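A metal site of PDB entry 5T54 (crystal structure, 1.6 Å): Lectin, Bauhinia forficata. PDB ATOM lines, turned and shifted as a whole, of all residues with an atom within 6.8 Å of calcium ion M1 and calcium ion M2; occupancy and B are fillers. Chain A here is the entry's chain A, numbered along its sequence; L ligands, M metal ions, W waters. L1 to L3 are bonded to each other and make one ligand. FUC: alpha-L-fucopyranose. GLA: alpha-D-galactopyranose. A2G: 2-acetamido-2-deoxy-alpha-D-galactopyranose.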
ATOM      1  N   ASP A  78      16.932 -26.081 -16.689  1.00  0.00           N
ATOM      2  CA  ASP A  78      16.459 -25.633 -18.016  1.00  0.00           C
ATOM      3  C   ASP A  78      17.266 -26.193 -19.185  1.00  0.00           C
ATOM      4  O   ASP A  78      16.811 -26.091 -20.357  1.00  0.00           O
ATOM      5  CB  ASP A  78      16.516 -24.121 -18.033  1.00  0.00           C
ATOM      6  CG  ASP A  78      15.271 -23.522 -17.416  1.00  0.00           C
ATOM      7  OD1 ASP A  78      14.279 -23.387 -18.168  1.00  0.00           O
ATOM      8  OD2 ASP A  78      15.328 -23.226 -16.158  1.00  0.00           O
ATOM      9  N   GLY A  95      17.193 -19.638 -15.579  1.00  0.00           N
ATOM     10  CA  GLY A  95      15.920 -20.099 -16.147  1.00  0.00           C
ATOM     11  C   GLY A  95      16.067 -20.384 -17.626  1.00  0.00           C
ATOM     12  O   GLY A  95      17.119 -20.825 -18.106  1.00  0.00           O
ATOM     13  N   GLY A  96      14.991 -20.154 -18.348  1.00  0.00           N
ATOM     14  CA  GLY A  96      14.883 -20.520 -19.770  1.00  0.00           C
ATOM     15  C   GLY A  96      15.840 -19.746 -20.666  1.00  0.00           C
ATOM     16  O   GLY A  96      16.012 -20.141 -21.829  1.00  0.00           O
ATOM     17  N   TYR A  97      16.370 -18.635 -20.178  1.00  0.00           N
ATOM     18  CA  TYR A  97      17.369 -17.867 -20.909  1.00  0.00           C
ATOM     19  C   TYR A  97      18.701 -18.619 -21.042  1.00  0.00           C
ATOM     20  O   TYR A  97      19.594 -18.116 -21.792  1.00  0.00           O
ATOM     21  CB  TYR A  97      17.573 -16.459 -20.286  1.00  0.00           C
ATOM     22  CG  TYR A  97      16.248 -15.750 -20.192  1.00  0.00           C
ATOM     23  CD1 TYR A  97      15.644 -15.231 -21.345  1.00  0.00           C
ATOM     24  CD2 TYR A  97      15.569 -15.661 -19.015  1.00  0.00           C
ATOM     25  CE1 TYR A  97      14.363 -14.652 -21.269  1.00  0.00           C
ATOM     26  CE2 TYR A  97      14.279 -15.103 -18.940  1.00  0.00           C
ATOM     27  CZ  TYR A  97      13.708 -14.578 -20.076  1.00  0.00           C
ATOM     28  OH  TYR A  97      12.470 -13.986 -20.062  1.00  0.00           O
ATOM     29  N   LEU A  98      18.917 -19.737 -20.314  1.00  0.00           N
ATOM     30  CA  LEU A  98      20.102 -20.617 -20.426  1.00  0.00           C
ATOM     31  C   LEU A  98      21.413 -19.935 -20.182  1.00  0.00           C
ATOM     32  O   LEU A  98      22.472 -20.390 -20.630  1.00  0.00           O
ATOM     33  CB  LEU A  98      20.088 -21.270 -21.863  1.00  0.00           C
ATOM     34  CG  LEU A  98      18.926 -22.220 -22.067  1.00  0.00           C
ATOM     35  CD1 LEU A  98      18.912 -22.774 -23.485  1.00  0.00           C
ATOM     36  CD2 LEU A  98      18.947 -23.327 -21.055  1.00  0.00           C
ATOM     37  N   GLU A 118      21.880 -25.538 -28.293  1.00  0.00           N
ATOM     38  CA  GLU A 118      21.204 -25.738 -27.017  1.00  0.00           C
ATOM     39  C   GLU A 118      20.600 -27.122 -26.839  1.00  0.00           C
ATOM     40  O   GLU A 118      20.154 -27.760 -27.810  1.00  0.00           O
ATOM     41  CB  GLU A 118      20.117 -24.648 -26.794  1.00  0.00           C
ATOM     42  CG  GLU A 118      18.963 -24.651 -27.744  1.00  0.00           C
ATOM     43  CD  GLU A 118      17.802 -23.809 -27.235  1.00  0.00           C
ATOM     44  OE1 GLU A 118      18.015 -22.583 -27.027  1.00  0.00           O
ATOM     45  OE2 GLU A 118      16.643 -24.289 -27.192  1.00  0.00           O
ATOM     46  N   ASP A 120      17.642 -28.336 -24.524  1.00  0.00           N
ATOM     47  CA  ASP A 120      16.607 -27.588 -23.790  1.00  0.00           C
ATOM     48  C   ASP A 120      15.645 -28.584 -23.127  1.00  0.00           C
ATOM     49  O   ASP A 120      14.914 -29.329 -23.791  1.00  0.00           O
ATOM     50  CB  ASP A 120      15.906 -26.631 -24.738  1.00  0.00           C
ATOM     51  CG  ASP A 120      14.982 -25.711 -24.044  1.00  0.00           C
ATOM     52  OD1 ASP A 120      14.489 -26.076 -22.959  1.00  0.00           O
ATOM     53  OD2 ASP A 120      14.685 -24.581 -24.575  1.00  0.00           O
ATOM     54  N   THR A 121      15.666 -28.640 -21.767  1.00  0.00           N
ATOM     55  CA  THR A 121      14.921 -29.594 -21.005  1.00  0.00           C
ATOM     56  C   THR A 121      13.576 -29.078 -20.532  1.00  0.00           C
ATOM     57  O   THR A 121      12.847 -29.879 -19.943  1.00  0.00           O
ATOM     58  CB  THR A 121      15.694 -30.047 -19.753  1.00  0.00           C
ATOM     59  OG1 THR A 121      16.017 -28.868 -18.923  1.00  0.00           O
ATOM     60  CG2 THR A 121      16.978 -30.814 -20.122  1.00  0.00           C
ATOM     61  N   TRP A 122      13.299 -27.789 -20.682  1.00  0.00           N
ATOM     62  CA  TRP A 122      12.055 -27.205 -20.136  1.00  0.00           C
ATOM     63  C   TRP A 122      11.346 -26.441 -21.236  1.00  0.00           C
ATOM     64  O   TRP A 122      11.913 -25.442 -21.753  1.00  0.00           O
ATOM     65  CB  TRP A 122      12.358 -26.268 -18.968  1.00  0.00           C
ATOM     66  CG  TRP A 122      11.143 -25.587 -18.407  1.00  0.00           C
ATOM     67  CD1 TRP A 122      10.636 -24.462 -18.904  1.00  0.00           C
ATOM     68  CD2 TRP A 122      10.298 -25.981 -17.309  1.00  0.00           C
ATOM     69  NE1 TRP A 122       9.495 -24.093 -18.207  1.00  0.00           N
ATOM     70  CE2 TRP A 122       9.293 -25.008 -17.209  1.00  0.00           C
ATOM     71  CE3 TRP A 122      10.278 -27.102 -16.439  1.00  0.00           C
ATOM     72  CZ2 TRP A 122       8.284 -25.044 -16.227  1.00  0.00           C
ATOM     73  CZ3 TRP A 122       9.299 -27.146 -15.431  1.00  0.00           C
ATOM     74  CH2 TRP A 122       8.314 -26.131 -15.347  1.00  0.00           C
ATOM     75  N   VAL A 123      10.139 -26.874 -21.574  1.00  0.00           N
ATOM     76  CA  VAL A 123       9.327 -26.168 -22.522  1.00  0.00           C
ATOM     77  C   VAL A 123       8.819 -24.777 -21.958  1.00  0.00           C
ATOM     78  O   VAL A 123       8.021 -24.729 -21.033  1.00  0.00           O
ATOM     79  CB  VAL A 123       8.130 -27.020 -23.003  1.00  0.00           C
ATOM     80  CG1 VAL A 123       7.185 -26.223 -23.860  1.00  0.00           C
ATOM     81  CG2 VAL A 123       8.643 -28.272 -23.692  1.00  0.00           C
ATOM     82  N   ASN A 124       9.315 -23.684 -22.565  1.00  0.00           N
ATOM     83  CA  ASN A 124       8.915 -22.356 -22.231  1.00  0.00           C
ATOM     84  C   ASN A 124       7.803 -21.844 -23.131  1.00  0.00           C
ATOM     85  O   ASN A 124       7.774 -22.076 -24.343  1.00  0.00           O
ATOM     86  CB  ASN A 124      10.093 -21.411 -22.351  1.00  0.00           C
ATOM     87  CG  ASN A 124      11.093 -21.627 -21.268  1.00  0.00           C
ATOM     88  OD1 ASN A 124      12.076 -22.303 -21.481  1.00  0.00           O
ATOM     89  ND2 ASN A 124      10.912 -20.970 -20.122  1.00  0.00           N
ATOM     90  N   TRP A 127       8.243 -17.436 -24.832  1.00  0.00           N
ATOM     91  CA  TRP A 127       8.646 -17.156 -26.234  1.00  0.00           C
ATOM     92  C   TRP A 127       8.313 -18.426 -27.002  1.00  0.00           C
ATOM     93  O   TRP A 127       7.944 -19.488 -26.408  1.00  0.00           O
ATOM     94  CB  TRP A 127      10.177 -16.889 -26.352  1.00  0.00           C
ATOM     95  CG  TRP A 127      11.012 -17.896 -25.618  1.00  0.00           C
ATOM     96  CD1 TRP A 127      11.512 -19.123 -26.085  1.00  0.00           C
ATOM     97  CD2 TRP A 127      11.513 -17.772 -24.296  1.00  0.00           C
ATOM     98  NE1 TRP A 127      12.230 -19.740 -25.099  1.00  0.00           N
ATOM     99  CE2 TRP A 127      12.264 -18.914 -24.010  1.00  0.00           C
ATOM    100  CE3 TRP A 127      11.385 -16.772 -23.299  1.00  0.00           C
ATOM    101  CZ2 TRP A 127      12.897 -19.094 -22.806  1.00  0.00           C
ATOM    102  CZ3 TRP A 127      12.028 -17.008 -22.081  1.00  0.00           C
ATOM    103  CH2 TRP A 127      12.764 -18.123 -21.850  1.00  0.00           C
ATOM    104  N   LYS A 128       8.425 -18.361 -28.311  1.00  0.00           N
ATOM    105  CA  LYS A 128       8.084 -19.462 -29.208  1.00  0.00           C
ATOM    106  C   LYS A 128       9.162 -20.556 -29.105  1.00  0.00           C
ATOM    107  O   LYS A 128      10.326 -20.299 -29.429  1.00  0.00           O
ATOM    108  CB  LYS A 128       8.030 -18.968 -30.677  1.00  0.00           C
ATOM    109  CG  LYS A 128       7.893 -20.114 -31.680  1.00  0.00           C
ATOM    110  CD  LYS A 128       7.460 -19.647 -33.080  1.00  0.00           C
ATOM    111  CE  LYS A 128       8.520 -18.782 -33.810  1.00  0.00           C
ATOM    112  NZ  LYS A 128       9.526 -19.628 -34.559  1.00  0.00           N
ATOM    113  N   GLU A 129       8.791 -21.747 -28.714  1.00  0.00           N
ATOM    114  CA  GLU A 129       9.659 -22.936 -28.913  1.00  0.00           C
ATOM    115  C   GLU A 129       8.784 -24.170 -28.923  1.00  0.00           C
ATOM    116  O   GLU A 129       7.518 -24.042 -28.670  1.00  0.00           O
ATOM    117  CB  GLU A 129      10.806 -23.030 -27.880  1.00  0.00           C
ATOM    118  CG  GLU A 129      10.381 -23.196 -26.425  1.00  0.00           C
ATOM    119  CD  GLU A 129      11.619 -23.153 -25.456  1.00  0.00           C
ATOM    120  OE1 GLU A 129      12.686 -22.617 -25.850  1.00  0.00           O
ATOM    121  OE2 GLU A 129      11.559 -23.754 -24.360  1.00  0.00           O
ATOM    122  N   PRO A 130       9.333 -25.299 -29.339  1.00  0.00           N
ATOM    123  CA  PRO A 130       8.454 -26.485 -29.485  1.00  0.00           C
ATOM    124  C   PRO A 130       7.837 -26.942 -28.190  1.00  0.00           C
ATOM    125  O   PRO A 130       8.359 -26.659 -27.092  1.00  0.00           O
ATOM    126  CB  PRO A 130       9.399 -27.581 -30.007  1.00  0.00           C
ATOM    127  CG  PRO A 130      10.565 -26.873 -30.525  1.00  0.00           C
ATOM    128  CD  PRO A 130      10.712 -25.624 -29.706  1.00  0.00           C
ATOM    129  N   HIS A 134      13.950 -30.387 -26.657  1.00  0.00           N
ATOM    130  CA  HIS A 134      14.468 -30.146 -27.969  1.00  0.00           C
ATOM    131  C   HIS A 134      15.913 -29.768 -27.915  1.00  0.00           C
ATOM    132  O   HIS A 134      16.413 -29.245 -26.940  1.00  0.00           O
ATOM    133  CB  HIS A 134      13.630 -29.084 -28.746  1.00  0.00           C
ATOM    134  CG  HIS A 134      13.450 -27.780 -28.013  1.00  0.00           C
ATOM    135  ND1 HIS A 134      12.447 -27.590 -27.086  1.00  0.00           N
ATOM    136  CD2 HIS A 134      14.152 -26.632 -28.051  1.00  0.00           C
ATOM    137  CE1 HIS A 134      12.545 -26.364 -26.596  1.00  0.00           C
ATOM    138  NE2 HIS A 134      13.552 -25.765 -27.200  1.00  0.00           N
ATOM    139  N   GLY A 136      18.486 -27.380 -30.331  1.00  0.00           N
ATOM    140  CA  GLY A 136      18.443 -26.329 -31.316  1.00  0.00           C
ATOM    141  C   GLY A 136      19.744 -25.630 -31.567  1.00  0.00           C
ATOM    142  O   GLY A 136      20.683 -25.663 -30.758  1.00  0.00           O
ATOM    143  N   ASP A 138      20.863 -21.709 -32.089  1.00  0.00           N
ATOM    144  CA  ASP A 138      20.451 -20.294 -31.688  1.00  0.00           C
ATOM    145  C   ASP A 138      21.380 -19.339 -32.337  1.00  0.00           C
ATOM    146  O   ASP A 138      22.612 -19.504 -32.258  1.00  0.00           O
ATOM    147  CB  ASP A 138      20.473 -20.122 -30.169  1.00  0.00           C
ATOM    148  CG  ASP A 138      19.550 -21.049 -29.478  1.00  0.00           C
ATOM    149  OD1 ASP A 138      18.611 -21.587 -30.091  1.00  0.00           O
ATOM    150  OD2 ASP A 138      19.702 -21.203 -28.230  1.00  0.00           O
ATOM    151  N   ILE A 142      16.953 -16.507 -28.284  1.00  0.00           N
ATOM    152  CA  ILE A 142      16.525 -17.693 -27.578  1.00  0.00           C
ATOM    153  C   ILE A 142      15.501 -18.521 -28.399  1.00  0.00           C
ATOM    154  O   ILE A 142      15.214 -19.645 -28.042  1.00  0.00           O
ATOM    155  CB  ILE A 142      15.995 -17.282 -26.178  1.00  0.00           C
ATOM    156  CG1 ILE A 142      15.986 -18.431 -25.172  1.00  0.00           C
ATOM    157  CG2 ILE A 142      14.614 -16.630 -26.291  1.00  0.00           C
ATOM    158  CD1 ILE A 142      17.268 -19.134 -24.887  1.00  0.00           C
ATOM    159  N   VAL A 143      14.934 -17.967 -29.422  1.00  0.00           N
ATOM    160  CA  VAL A 143      14.024 -18.665 -30.374  1.00  0.00           C
ATOM    161  C   VAL A 143      14.970 -19.265 -31.429  1.00  0.00           C
ATOM    162  O   VAL A 143      15.457 -18.543 -32.307  1.00  0.00           O
ATOM    163  CB  VAL A 143      12.992 -17.685 -30.978  1.00  0.00           C
ATOM    164  CG1 VAL A 143      12.076 -18.413 -31.972  1.00  0.00           C
ATOM    165  CG2 VAL A 143      12.125 -17.144 -29.832  1.00  0.00           C
ATOM    166  N   SER A 144      15.089 -20.571 -31.386  1.00  0.00           N
ATOM    167  CA  SER A 144      16.076 -21.325 -32.202  1.00  0.00           C
ATOM    168  C   SER A 144      15.720 -21.195 -33.702  1.00  0.00           C
ATOM    169  O   SER A 144      14.543 -21.169 -34.073  1.00  0.00           O
ATOM    170  CB  SER A 144      16.051 -22.806 -31.871  1.00  0.00           C
ATOM    171  OG  SER A 144      16.368 -23.043 -30.501  1.00  0.00           O
ATOM    172  N   VAL A 147      15.494 -26.403 -35.002  1.00  0.00           N
ATOM    173  CA  VAL A 147      15.160 -27.084 -33.772  1.00  0.00           C
ATOM    174  C   VAL A 147      14.570 -28.444 -34.033  1.00  0.00           C
ATOM    175  O   VAL A 147      13.788 -28.610 -35.018  1.00  0.00           O
ATOM    176  CB  VAL A 147      14.202 -26.154 -32.963  1.00  0.00           C
ATOM    177  CG1 VAL A 147      12.804 -26.165 -33.578  1.00  0.00           C
ATOM    178  CG2 VAL A 147      14.195 -26.547 -31.530  1.00  0.00           C
HETATM  179  C1  FUC L   1       5.968 -20.965 -17.350  1.00  0.00           C
HETATM  180  C2  FUC L   1       6.303 -21.658 -18.665  1.00  0.00           C
HETATM  181  C3  FUC L   1       5.649 -23.028 -18.776  1.00  0.00           C
HETATM  182  C4  FUC L   1       4.129 -22.968 -18.467  1.00  0.00           C
HETATM  183  C5  FUC L   1       4.022 -22.269 -17.131  1.00  0.00           C
HETATM  184  C6  FUC L   1       2.564 -22.244 -16.622  1.00  0.00           C
HETATM  185  O2  FUC L   1       7.750 -21.678 -18.807  1.00  0.00           O
HETATM  186  O3  FUC L   1       5.805 -23.439 -20.127  1.00  0.00           O
HETATM  187  O4  FUC L   1       3.513 -22.292 -19.544  1.00  0.00           O
HETATM  188  O5  FUC L   1       4.530 -20.945 -17.247  1.00  0.00           O
HETATM  189  C1  GLA L   2       5.495 -20.882 -14.187  1.00  0.00           C
HETATM  190  C2  GLA L   2       6.629 -20.659 -15.144  1.00  0.00           C
HETATM  191  C3  GLA L   2       7.940 -20.856 -14.431  1.00  0.00           C
HETATM  192  C4  GLA L   2       7.969 -20.085 -13.137  1.00  0.00           C
HETATM  193  C5  GLA L   2       6.794 -20.342 -12.230  1.00  0.00           C
HETATM  194  C6  GLA L   2       6.814 -19.380 -11.024  1.00  0.00           C
HETATM  195  O1  GLA L   2       5.527 -22.252 -13.834  1.00  0.00           O
HETATM  196  O2  GLA L   2       6.604 -21.598 -16.228  1.00  0.00           O
HETATM  197  O3  GLA L   2       9.059 -20.533 -15.311  1.00  0.00           O
HETATM  198  O4  GLA L   2       7.952 -18.737 -13.527  1.00  0.00           O
HETATM  199  O5  GLA L   2       5.608 -20.073 -12.998  1.00  0.00           O
HETATM  200  O6  GLA L   2       5.755 -19.904 -10.188  1.00  0.00           O
HETATM  201  O5  A2G L   3      10.713 -21.549 -13.970  1.00  0.00           O
HETATM  202  C1  A2G L   3      10.374 -20.464 -14.828  1.00  0.00           C
HETATM  203  C2  A2G L   3      11.312 -20.336 -16.023  1.00  0.00           C
HETATM  204  N2  A2G L   3      10.865 -19.238 -16.823  1.00  0.00           N
HETATM  205  C3  A2G L   3      11.413 -21.650 -16.732  1.00  0.00           C
HETATM  206  O3  A2G L   3      12.402 -21.479 -17.762  1.00  0.00           O
HETATM  207  C4  A2G L   3      11.788 -22.735 -15.712  1.00  0.00           C
HETATM  208  O4  A2G L   3      13.073 -22.563 -15.084  1.00  0.00           O
HETATM  209  C5  A2G L   3      10.694 -22.802 -14.647  1.00  0.00           C
HETATM  210  C6  A2G L   3      10.972 -23.890 -13.618  1.00  0.00           C
HETATM  211  O6  A2G L   3       9.858 -23.908 -12.681  1.00  0.00           O
HETATM  212  C7  A2G L   3      11.710 -18.392 -17.376  1.00  0.00           C
HETATM  213  O7  A2G L   3      12.929 -18.442 -17.159  1.00  0.00           O
HETATM  214  C8  A2G L   3      11.138 -17.377 -18.338  1.00  0.00           C
HETATM  215 CA    CA M   1      14.605 -23.696 -26.632  1.00  0.00          CA
HETATM  216 CA    CA M   2      13.310 -23.822 -22.729  1.00  0.00          CA
HETATM  217  O   HOH W   1      14.357 -23.225 -28.873  1.00  0.00           O
HETATM  218  O   HOH W   2      14.625 -21.876 -23.392  1.00  0.00           O
HETATM  219  O   HOH W   3      15.624 -21.726 -26.184  1.00  0.00           O
HETATM  220  O   HOH W   4      14.685 -24.013 -20.740  1.00  0.00           O
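Calcium ion M2 is bound by the side-chain amide oxygen (OD1) of Asn 124 (2.3 Å), the backbone carbonyl oxygen (O) of Trp 122 (2.4 Å), the side-chain carboxylate (OE2) of Glu 129 (2.4 Å), the side-chain carboxylate (OD2) of Asp 120 (2.4 Å), water W4 (2.4 Å), water W2 (2.4 Å) and the side-chain carboxylate (OD1) of Asp 120 (2.6 Å).
The side-chain carboxylate of Asp 138 lies close to the side-chain carboxylate of Glu 118 (2.5 Å).
O of Gly 136 is in hydrogen-bond range of N of Glu 118, at 2.7 Å.
OE1 of Glu 129 sits close to NE1 of Trp 127.
Water W3 lies within hydrogen-bond range of OE1 of Glu 118 (2.7 Å) and O of Ile 142 (2.8 Å).
OE2 of Glu 118 is bound to calcium ion M1 (2.2 Å).
OD2 of Asp 120 is bound to calcium ion M1.
Calcium ion M1 is bound by water W3.
Water W1 is bound to calcium ion M1 (2.3 Å).
Calcium ion M1 is bound by OE1 of Glu 129 (2.3 Å).
Calcium ion M1 is bound by a ring nitrogen (NE2) of His 134 (2.4 Å).
Calcium ion M1 has six donor atoms within binding distance.
Four residues have an atom within 4 Å of calcium ion M2: Asp 120, Trp 122, Asn 124 and Glu 129.
OD2 of Asp 78 sits at hydrogen-bond distance from O4 of A2G L3 (2.6 Å).
The side-chain amide nitrogen of Asn 124 is in hydrogen-bond range of an oxygen (O3) of A2G L3 (2.8 Å).
O2 of FUC L1 is in hydrogen-bond range of NE1 of Trp 122, 3.0 Å away.
O of Val 123 lies within hydrogen-bond range of O3 of FUC L1, at 2.7 Å.
N of Gly 96 lies within hydrogen-bond range of O7 of A2G L3, 2.9 Å away.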
